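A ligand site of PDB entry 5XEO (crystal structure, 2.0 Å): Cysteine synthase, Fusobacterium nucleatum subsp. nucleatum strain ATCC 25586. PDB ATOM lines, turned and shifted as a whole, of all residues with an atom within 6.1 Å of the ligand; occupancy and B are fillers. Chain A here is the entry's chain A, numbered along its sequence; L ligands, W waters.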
ATOM      1  N   SER A  44      21.212   6.872 -24.647  1.00  0.00           N
ATOM      2  CA  SER A  44      20.214   5.809 -24.674  1.00  0.00           C
ATOM      3  C   SER A  44      20.108   5.103 -23.346  1.00  0.00           C
ATOM      4  O   SER A  44      20.982   5.232 -22.479  1.00  0.00           O
ATOM      5  CB  SER A  44      20.530   4.787 -25.785  1.00  0.00           C
ATOM      6  OG  SER A  44      21.381   3.721 -25.345  1.00  0.00           O
ATOM      7  N   THR A  45      19.038   4.321 -23.208  1.00  0.00           N
ATOM      8  CA  THR A  45      18.803   3.516 -22.039  1.00  0.00           C
ATOM      9  C   THR A  45      19.886   2.444 -21.871  1.00  0.00           C
ATOM     10  O   THR A  45      20.071   1.935 -20.784  1.00  0.00           O
ATOM     11  CB  THR A  45      17.402   2.846 -22.074  1.00  0.00           C
ATOM     12  OG1 THR A  45      16.943   2.700 -20.756  1.00  0.00           O
ATOM     13  CG2 THR A  45      17.393   1.462 -22.764  1.00  0.00           C
ATOM     14  N   LYS A  46      20.567   2.084 -22.956  1.00  0.00           N
ATOM     15  CA  LYS A  46      21.564   1.035 -22.912  1.00  0.00           C
ATOM     16  C   LYS A  46      22.749   1.366 -22.008  1.00  0.00           C
ATOM     17  O   LYS A  46      23.427   0.437 -21.550  1.00  0.00           O
ATOM     18  CB  LYS A  46      22.058   0.639 -24.287  1.00  0.00           C
ATOM     19  CG  LYS A  46      20.988   0.259 -25.292  1.00  0.00           C
ATOM     20  CD  LYS A  46      20.160  -0.951 -24.832  1.00  0.00           C
ATOM     21  CE  LYS A  46      18.922  -1.136 -25.656  1.00  0.00           C
ATOM     22  NZ  LYS A  46      19.114  -1.166 -27.115  1.00  0.00           N
ATOM     23  N   ILE A  49      22.293  -0.717 -18.866  1.00  0.00           N
ATOM     24  CA  ILE A  49      22.613  -2.135 -18.968  1.00  0.00           C
ATOM     25  C   ILE A  49      24.127  -2.349 -19.196  1.00  0.00           C
ATOM     26  O   ILE A  49      24.709  -3.302 -18.668  1.00  0.00           O
ATOM     27  CB  ILE A  49      21.730  -2.930 -19.985  1.00  0.00           C
ATOM     28  CG1 ILE A  49      22.114  -2.665 -21.446  1.00  0.00           C
ATOM     29  CG2 ILE A  49      20.252  -2.689 -19.691  1.00  0.00           C
ATOM     30  CD1 ILE A  49      21.501  -3.660 -22.437  1.00  0.00           C
ATOM     31  N   GLY A  75      24.444  -1.450 -32.352  1.00  0.00           N
ATOM     32  CA  GLY A  75      23.565  -0.444 -31.799  1.00  0.00           C
ATOM     33  C   GLY A  75      24.016   0.313 -30.557  1.00  0.00           C
ATOM     34  O   GLY A  75      25.207   0.413 -30.251  1.00  0.00           O
ATOM     35  N   ASN A  76      23.016   0.811 -29.828  1.00  0.00           N
ATOM     36  CA  ASN A  76      23.231   1.596 -28.659  1.00  0.00           C
ATOM     37  C   ASN A  76      23.982   0.888 -27.552  1.00  0.00           C
ATOM     38  O   ASN A  76      24.693   1.535 -26.779  1.00  0.00           O
ATOM     39  CB  ASN A  76      21.915   2.109 -28.120  1.00  0.00           C
ATOM     40  CG  ASN A  76      21.411   3.313 -28.918  1.00  0.00           C
ATOM     41  OD1 ASN A  76      22.204   4.203 -29.283  1.00  0.00           O
ATOM     42  ND2 ASN A  76      20.108   3.357 -29.172  1.00  0.00           N
ATOM     43  N   THR A  77      23.843  -0.444 -27.485  1.00  0.00           N
ATOM     44  CA  THR A  77      24.624  -1.160 -26.484  1.00  0.00           C
ATOM     45  C   THR A  77      26.141  -1.000 -26.644  1.00  0.00           C
ATOM     46  O   THR A  77      26.840  -0.866 -25.658  1.00  0.00           O
ATOM     47  CB  THR A  77      24.202  -2.627 -26.431  1.00  0.00           C
ATOM     48  OG1 THR A  77      22.873  -2.651 -25.942  1.00  0.00           O
ATOM     49  CG2 THR A  77      25.107  -3.407 -25.440  1.00  0.00           C
ATOM     50  N   GLN A 146      24.063  -8.968 -24.222  1.00  0.00           N
ATOM     51  CA  GLN A 146      22.812  -8.291 -23.824  1.00  0.00           C
ATOM     52  C   GLN A 146      21.547  -9.148 -23.992  1.00  0.00           C
ATOM     53  O   GLN A 146      20.551  -8.937 -23.293  1.00  0.00           O
ATOM     54  CB  GLN A 146      22.638  -6.997 -24.603  1.00  0.00           C
ATOM     55  CG  GLN A 146      22.517  -7.169 -26.104  1.00  0.00           C
ATOM     56  CD  GLN A 146      22.376  -5.835 -26.816  1.00  0.00           C
ATOM     57  OE1 GLN A 146      21.819  -4.881 -26.263  1.00  0.00           O
ATOM     58  NE2 GLN A 146      22.874  -5.771 -28.021  1.00  0.00           N
ATOM     59  N   ASN A 152      20.863  -7.109 -17.831  1.00  0.00           N
ATOM     60  CA  ASN A 152      20.081  -6.248 -18.718  1.00  0.00           C
ATOM     61  C   ASN A 152      18.718  -5.949 -18.078  1.00  0.00           C
ATOM     62  O   ASN A 152      18.500  -4.809 -17.600  1.00  0.00           O
ATOM     63  CB  ASN A 152      20.083  -6.843 -20.162  1.00  0.00           C
ATOM     64  CG  ASN A 152      19.089  -6.188 -21.095  1.00  0.00           C
ATOM     65  OD1 ASN A 152      18.320  -5.277 -20.711  1.00  0.00           O
ATOM     66  ND2 ASN A 152      19.090  -6.657 -22.328  1.00  0.00           N
ATOM     67  N   HIS A 156      16.995  -2.331 -15.238  1.00  0.00           N
ATOM     68  CA  HIS A 156      15.725  -1.636 -15.389  1.00  0.00           C
ATOM     69  C   HIS A 156      14.741  -1.906 -14.230  1.00  0.00           C
ATOM     70  O   HIS A 156      14.048  -0.995 -13.761  1.00  0.00           O
ATOM     71  CB  HIS A 156      15.107  -2.072 -16.717  1.00  0.00           C
ATOM     72  CG  HIS A 156      15.877  -1.607 -17.897  1.00  0.00           C
ATOM     73  ND1 HIS A 156      16.001  -0.268 -18.213  1.00  0.00           N
ATOM     74  CD2 HIS A 156      16.541  -2.279 -18.858  1.00  0.00           C
ATOM     75  CE1 HIS A 156      16.702  -0.148 -19.324  1.00  0.00           C
ATOM     76  NE2 HIS A 156      17.024  -1.349 -19.746  1.00  0.00           N
ATOM     77  N   CYS A 177       6.551   0.106 -23.925  1.00  0.00           N
ATOM     78  CA  CYS A 177       8.010   0.077 -24.161  1.00  0.00           C
ATOM     79  C   CYS A 177       8.336  -0.705 -25.393  1.00  0.00           C
ATOM     80  O   CYS A 177       7.809  -1.799 -25.578  1.00  0.00           O
ATOM     81  CB  CYS A 177       8.660  -0.588 -22.938  1.00  0.00           C
ATOM     82  SG  CYS A 177      10.450  -0.512 -22.880  1.00  0.00           S
ATOM     83  N   GLY A 178       9.215  -0.165 -26.261  1.00  0.00           N
ATOM     84  CA  GLY A 178       9.685  -0.892 -27.426  1.00  0.00           C
ATOM     85  C   GLY A 178      10.572  -2.080 -27.058  1.00  0.00           C
ATOM     86  O   GLY A 178      11.173  -2.084 -25.996  1.00  0.00           O
ATOM     87  N   THR A 179      10.639  -3.099 -27.920  1.00  0.00           N
ATOM     88  CA  THR A 179      11.454  -4.270 -27.641  1.00  0.00           C
ATOM     89  C   THR A 179      12.446  -4.559 -28.725  1.00  0.00           C
ATOM     90  O   THR A 179      12.153  -4.402 -29.922  1.00  0.00           O
ATOM     91  CB  THR A 179      10.599  -5.560 -27.421  1.00  0.00           C
ATOM     92  OG1 THR A 179       9.823  -5.847 -28.597  1.00  0.00           O
ATOM     93  CG2 THR A 179       9.735  -5.392 -26.283  1.00  0.00           C
ATOM     94  N   GLY A 180      13.633  -4.955 -28.274  1.00  0.00           N
ATOM     95  CA  GLY A 180      14.701  -5.489 -29.089  1.00  0.00           C
ATOM     96  C   GLY A 180      15.250  -6.707 -28.363  1.00  0.00           C
ATOM     97  O   GLY A 180      14.931  -7.839 -28.730  1.00  0.00           O
ATOM     98  N   THR A 181      16.037  -6.477 -27.310  1.00  0.00           N
ATOM     99  CA  THR A 181      16.359  -7.573 -26.397  1.00  0.00           C
ATOM    100  C   THR A 181      15.165  -7.987 -25.568  1.00  0.00           C
ATOM    101  O   THR A 181      15.048  -9.140 -25.158  1.00  0.00           O
ATOM    102  CB  THR A 181      17.505  -7.241 -25.422  1.00  0.00           C
ATOM    103  OG1 THR A 181      17.063  -6.264 -24.469  1.00  0.00           O
ATOM    104  CG2 THR A 181      18.736  -6.799 -26.185  1.00  0.00           C
ATOM    105  N   GLY A 182      14.285  -7.033 -25.294  1.00  0.00           N
ATOM    106  CA  GLY A 182      13.179  -7.208 -24.407  1.00  0.00           C
ATOM    107  C   GLY A 182      13.495  -6.891 -22.969  1.00  0.00           C
ATOM    108  O   GLY A 182      12.625  -7.009 -22.104  1.00  0.00           O
ATOM    109  N   GLY A 183      14.707  -6.416 -22.678  1.00  0.00           N
ATOM    110  CA  GLY A 183      15.135  -6.204 -21.306  1.00  0.00           C
ATOM    111  C   GLY A 183      14.532  -5.010 -20.629  1.00  0.00           C
ATOM    112  O   GLY A 183      14.151  -5.100 -19.457  1.00  0.00           O
ATOM    113  N   SER A 184      14.452  -3.874 -21.333  1.00  0.00           N
ATOM    114  CA  SER A 184      13.850  -2.691 -20.750  1.00  0.00           C
ATOM    115  C   SER A 184      12.375  -2.920 -20.465  1.00  0.00           C
ATOM    116  O   SER A 184      11.891  -2.555 -19.378  1.00  0.00           O
ATOM    117  CB  SER A 184      14.049  -1.430 -21.627  1.00  0.00           C
ATOM    118  OG  SER A 184      13.566  -1.646 -22.917  1.00  0.00           O
ATOM    119  N   PHE A 185      11.662  -3.541 -21.403  1.00  0.00           N
ATOM    120  CA  PHE A 185      10.250  -3.882 -21.131  1.00  0.00           C
ATOM    121  C   PHE A 185      10.116  -4.831 -19.921  1.00  0.00           C
ATOM    122  O   PHE A 185       9.357  -4.578 -18.967  1.00  0.00           O
ATOM    123  CB  PHE A 185       9.578  -4.566 -22.332  1.00  0.00           C
ATOM    124  CG  PHE A 185       8.257  -5.180 -21.963  1.00  0.00           C
ATOM    125  CD1 PHE A 185       7.166  -4.372 -21.665  1.00  0.00           C
ATOM    126  CD2 PHE A 185       8.140  -6.561 -21.785  1.00  0.00           C
ATOM    127  CE1 PHE A 185       5.948  -4.919 -21.261  1.00  0.00           C
ATOM    128  CE2 PHE A 185       6.926  -7.121 -21.383  1.00  0.00           C
ATOM    129  CZ  PHE A 185       5.845  -6.301 -21.101  1.00  0.00           C
ATOM    130  N   GLN A 223      15.010   1.273 -35.874  1.00  0.00           N
ATOM    131  CA  GLN A 223      16.348   0.924 -35.334  1.00  0.00           C
ATOM    132  C   GLN A 223      16.325   0.681 -33.815  1.00  0.00           C
ATOM    133  O   GLN A 223      15.733   1.456 -33.036  1.00  0.00           O
ATOM    134  CB  GLN A 223      17.385   1.976 -35.704  1.00  0.00           C
ATOM    135  CG  GLN A 223      17.742   1.913 -37.187  1.00  0.00           C
ATOM    136  CD  GLN A 223      18.796   2.918 -37.615  1.00  0.00           C
ATOM    137  OE1 GLN A 223      19.865   3.025 -36.993  1.00  0.00           O
ATOM    138  NE2 GLN A 223      18.531   3.634 -38.713  1.00  0.00           N
ATOM    139  N   GLY A 224      16.926  -0.433 -33.403  1.00  0.00           N
ATOM    140  CA  GLY A 224      16.966  -0.867 -32.009  1.00  0.00           C
ATOM    141  C   GLY A 224      15.857  -1.816 -31.627  1.00  0.00           C
ATOM    142  O   GLY A 224      15.962  -2.551 -30.632  1.00  0.00           O
ATOM    143  N   MET A 225      14.747  -1.819 -32.371  1.00  0.00           N
ATOM    144  CA  MET A 225      13.677  -2.740 -32.062  1.00  0.00           C
ATOM    145  C   MET A 225      13.761  -3.938 -33.019  1.00  0.00           C
ATOM    146  O   MET A 225      14.558  -3.951 -33.931  1.00  0.00           O
ATOM    147  CB  MET A 225      12.325  -2.036 -32.140  1.00  0.00           C
ATOM    148  CG  MET A 225      11.966  -1.205 -30.908  1.00  0.00           C
ATOM    149  SD  MET A 225      10.459  -0.193 -31.045  1.00  0.00           S
ATOM    150  CE  MET A 225       9.346  -1.429 -31.731  1.00  0.00           C
ATOM    151  N   GLY A 268      14.457   8.951 -30.869  1.00  0.00           N
ATOM    152  CA  GLY A 268      14.803   8.101 -31.970  1.00  0.00           C
ATOM    153  C   GLY A 268      13.563   7.532 -32.636  1.00  0.00           C
ATOM    154  O   GLY A 268      12.422   7.845 -32.273  1.00  0.00           O
ATOM    155  N   SER A 270      12.556   4.439 -32.520  1.00  0.00           N
ATOM    156  CA  SER A 270      11.812   3.572 -31.614  1.00  0.00           C
ATOM    157  C   SER A 270      10.918   4.359 -30.689  1.00  0.00           C
ATOM    158  O   SER A 270       9.915   3.830 -30.213  1.00  0.00           O
ATOM    159  CB  SER A 270      12.732   2.594 -30.818  1.00  0.00           C
ATOM    160  OG  SER A 270      13.445   3.226 -29.768  1.00  0.00           O
ATOM    161  N   THR A 271      11.294   5.606 -30.375  1.00  0.00           N
ATOM    162  CA  THR A 271      10.463   6.469 -29.537  1.00  0.00           C
ATOM    163  C   THR A 271       9.184   6.842 -30.319  1.00  0.00           C
ATOM    164  O   THR A 271       8.091   6.830 -29.787  1.00  0.00           O
ATOM    165  CB  THR A 271      11.237   7.727 -29.102  1.00  0.00           C
ATOM    166  OG1 THR A 271      12.329   7.344 -28.241  1.00  0.00           O
ATOM    167  CG2 THR A 271      10.342   8.698 -28.413  1.00  0.00           C
ATOM    168  N   THR A 297      13.617   5.402 -25.759  1.00  0.00           N
ATOM    169  CA  THR A 297      14.842   4.650 -25.561  1.00  0.00           C
ATOM    170  C   THR A 297      16.116   5.418 -25.907  1.00  0.00           C
ATOM    171  O   THR A 297      17.096   5.255 -25.201  1.00  0.00           O
ATOM    172  CB  THR A 297      14.782   3.262 -26.233  1.00  0.00           C
ATOM    173  OG1 THR A 297      13.659   2.556 -25.662  1.00  0.00           O
ATOM    174  CG2 THR A 297      16.054   2.452 -25.983  1.00  0.00           C
ATOM    175  N   ASP A 298      16.109   6.249 -26.947  1.00  0.00           N
ATOM    176  CA  ASP A 298      17.283   7.076 -27.239  1.00  0.00           C
ATOM    177  C   ASP A 298      16.857   8.401 -27.829  1.00  0.00           C
ATOM    178  O   ASP A 298      15.691   8.595 -28.151  1.00  0.00           O
ATOM    179  CB  ASP A 298      18.330   6.346 -28.103  1.00  0.00           C
ATOM    180  CG  ASP A 298      17.941   6.163 -29.548  1.00  0.00           C
ATOM    181  OD1 ASP A 298      16.736   6.278 -29.877  1.00  0.00           O
ATOM    182  OD2 ASP A 298      18.833   5.825 -30.351  1.00  0.00           O
ATOM    183  N   TYR A 303      19.849   9.724 -35.951  1.00  0.00           N
ATOM    184  CA  TYR A 303      19.020   9.282 -37.089  1.00  0.00           C
ATOM    185  C   TYR A 303      18.751  10.403 -38.075  1.00  0.00           C
ATOM    186  O   TYR A 303      18.148  10.149 -39.106  1.00  0.00           O
ATOM    187  CB  TYR A 303      17.681   8.733 -36.619  1.00  0.00           C
ATOM    188  CG  TYR A 303      17.829   7.677 -35.566  1.00  0.00           C
ATOM    189  CD1 TYR A 303      18.276   6.394 -35.900  1.00  0.00           C
ATOM    190  CD2 TYR A 303      17.640   7.982 -34.218  1.00  0.00           C
ATOM    191  CE1 TYR A 303      18.455   5.431 -34.913  1.00  0.00           C
ATOM    192  CE2 TYR A 303      17.813   7.024 -33.236  1.00  0.00           C
ATOM    193  CZ  TYR A 303      18.222   5.738 -33.587  1.00  0.00           C
ATOM    194  OH  TYR A 303      18.407   4.770 -32.612  1.00  0.00           O
HETATM  195  N1  LIG L   1      15.161   1.480 -29.080  1.00  0.00           N
HETATM  196  C1  LIG L   1      16.517   1.700 -29.230  1.00  0.00           C
HETATM  197  C2  LIG L   1      16.992   2.987 -29.860  1.00  0.00           C
HETATM  198  C3  LIG L   1      17.422   0.769 -28.695  1.00  0.00           C
HETATM  199  O1  LIG L   1      18.737   0.991 -28.792  1.00  0.00           O
HETATM  200  C4  LIG L   1      16.978  -0.428 -28.114  1.00  0.00           C
HETATM  201  C5  LIG L   1      17.922  -1.507 -27.608  1.00  0.00           C
HETATM  202  C6  LIG L   1      15.590  -0.652 -28.011  1.00  0.00           C
HETATM  203  C7  LIG L   1      14.703   0.317 -28.501  1.00  0.00           C
HETATM  204  C8  LIG L   1      15.049  -1.908 -27.382  1.00  0.00           C
HETATM  205  O2  LIG L   1      15.278  -2.037 -25.954  1.00  0.00           O
HETATM  206  P1  LIG L   1      15.517  -3.450 -25.259  1.00  0.00           P
HETATM  207  O3  LIG L   1      15.571  -3.066 -23.838  1.00  0.00           O
HETATM  208  O4  LIG L   1      16.674  -4.066 -25.945  1.00  0.00           O
HETATM  209  O5  LIG L   1      14.261  -4.278 -25.522  1.00  0.00           O
HETATM  210  O   HOH W   1      12.186  -4.079 -24.112  1.00  0.00           O
HETATM  211  O   HOH W   2      15.446   4.231 -32.741  1.00  0.00           O
HETATM  212  O   HOH W   3      17.676  -2.849 -22.175  1.00  0.00           O
HETATM  213  O   HOH W   4      20.274   0.384 -30.803  1.00  0.00           O
HETATM  214  O   HOH W   5      13.299   0.105 -24.918  1.00  0.00           O
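The backbone NH (N) of Lys 46 is in hydrogen-bond range of the side-chain hydroxyl (OG) of Ser 44 (3.0 Å). OG of Ser 184 lies within hydrogen-bond range of SG of Cys 177 (3.3 Å). N of Gly 183 sits at hydrogen-bond distance from OG1 of Thr 181, 3.0 Å away. The side-chain hydroxyl (OG1) of Thr 181 sits at hydrogen-bond distance from the side-chain amide nitrogen (ND2) of Asn 152, at 3.0 Å. OD2 of Asp 298 lies within hydrogen-bond range of OH of Tyr 303 (2.5 Å). The backbone NH (N) of Gly 268 lies within hydrogen-bond range of the backbone carbonyl oxygen (O) of Asp 298, at 3.0 Å. N of Thr 45 lies within hydrogen-bond range of O of Thr 297 (2.9 Å). OG1 of Thr 271 lies within hydrogen-bond range of N of Thr 297 (3.4 Å).
Water W1 lies within hydrogen-bond range of an oxygen (O5) of the ligand, the backbone NH (N) of Phe 185, the backbone carbonyl oxygen (O) of Gly 178 and the side-chain hydroxyl (OG) of Ser 184. Water W4 bridges O1 of the ligand (2.6 Å) and N of Asn 76 (2.9 Å). Water W3 lies within hydrogen-bond range of an oxygen (O3) of the ligand, the side-chain amide oxygen of Asn 152, a ring nitrogen (NE2) of His 156 and the backbone NH of Ser 184. Water W5 lies within hydrogen-bond range of the side-chain hydroxyl of Thr 297, the side-chain hydroxyl of Ser 184, an oxygen (O2) of the ligand, the backbone carbonyl oxygen of Gly 178 and the side-chain sulfur of Cys 177. Water W2 lies within hydrogen-bond range of O of Gln 223, N of Ser 270 and OH of Tyr 303.
Gly 178 touches the ligand (O to O5, 3.8 Å). Thr 179 touches the ligand (CA to O5, 3.5 Å). Gly 183 touches the ligand (N to O5, 3.6 Å). O of Gln 223 touches C2 of the ligand, at 3.7 Å. Gly 224 touches the ligand. Met 225 touches the ligand (CG to C7, 3.9 Å). Thr 297 touches the ligand. OD1 of Asp 298 touches C2 of the ligand, at 3.3 Å. OH of Tyr 303 touches C2 of the ligand, at 3.6 Å. Hydrophobic or aromatic side chains within 4 Å of the ligand: Met 225. Of the 28 residues printed, 16 come within 4 Å of the ligand.
A carbon (C5) of the ligand is bonded to the side-chain amino group (NZ) of Lys 46, at 1.3 Å. OG of Ser 270 lies within hydrogen-bond range of N1 of the ligand (2.5 Å). The backbone NH (N) of Ser 184 is in hydrogen-bond range of an oxygen (O3) of the ligand, at 2.9 Å. An oxygen (O3) of the ligand sits at hydrogen-bond distance from the side-chain hydroxyl (OG) of Ser 184 (2.6 Å). O4 of the ligand lies within hydrogen-bond range of N of Thr 181 (2.8 Å). O4 of the ligand lies within hydrogen-bond range of OG1 of Thr 181, 2.7 Å away. ND2 of Asn 76 is in hydrogen-bond range of O1 of the ligand (2.8 Å). The backbone NH (N) of Gly 182 sits at hydrogen-bond distance from an oxygen (O5) of the ligand, 2.8 Å away. An oxygen (O5) of the ligand is in hydrogen-bond range of the backbone NH of Gly 180 (2.9 Å).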
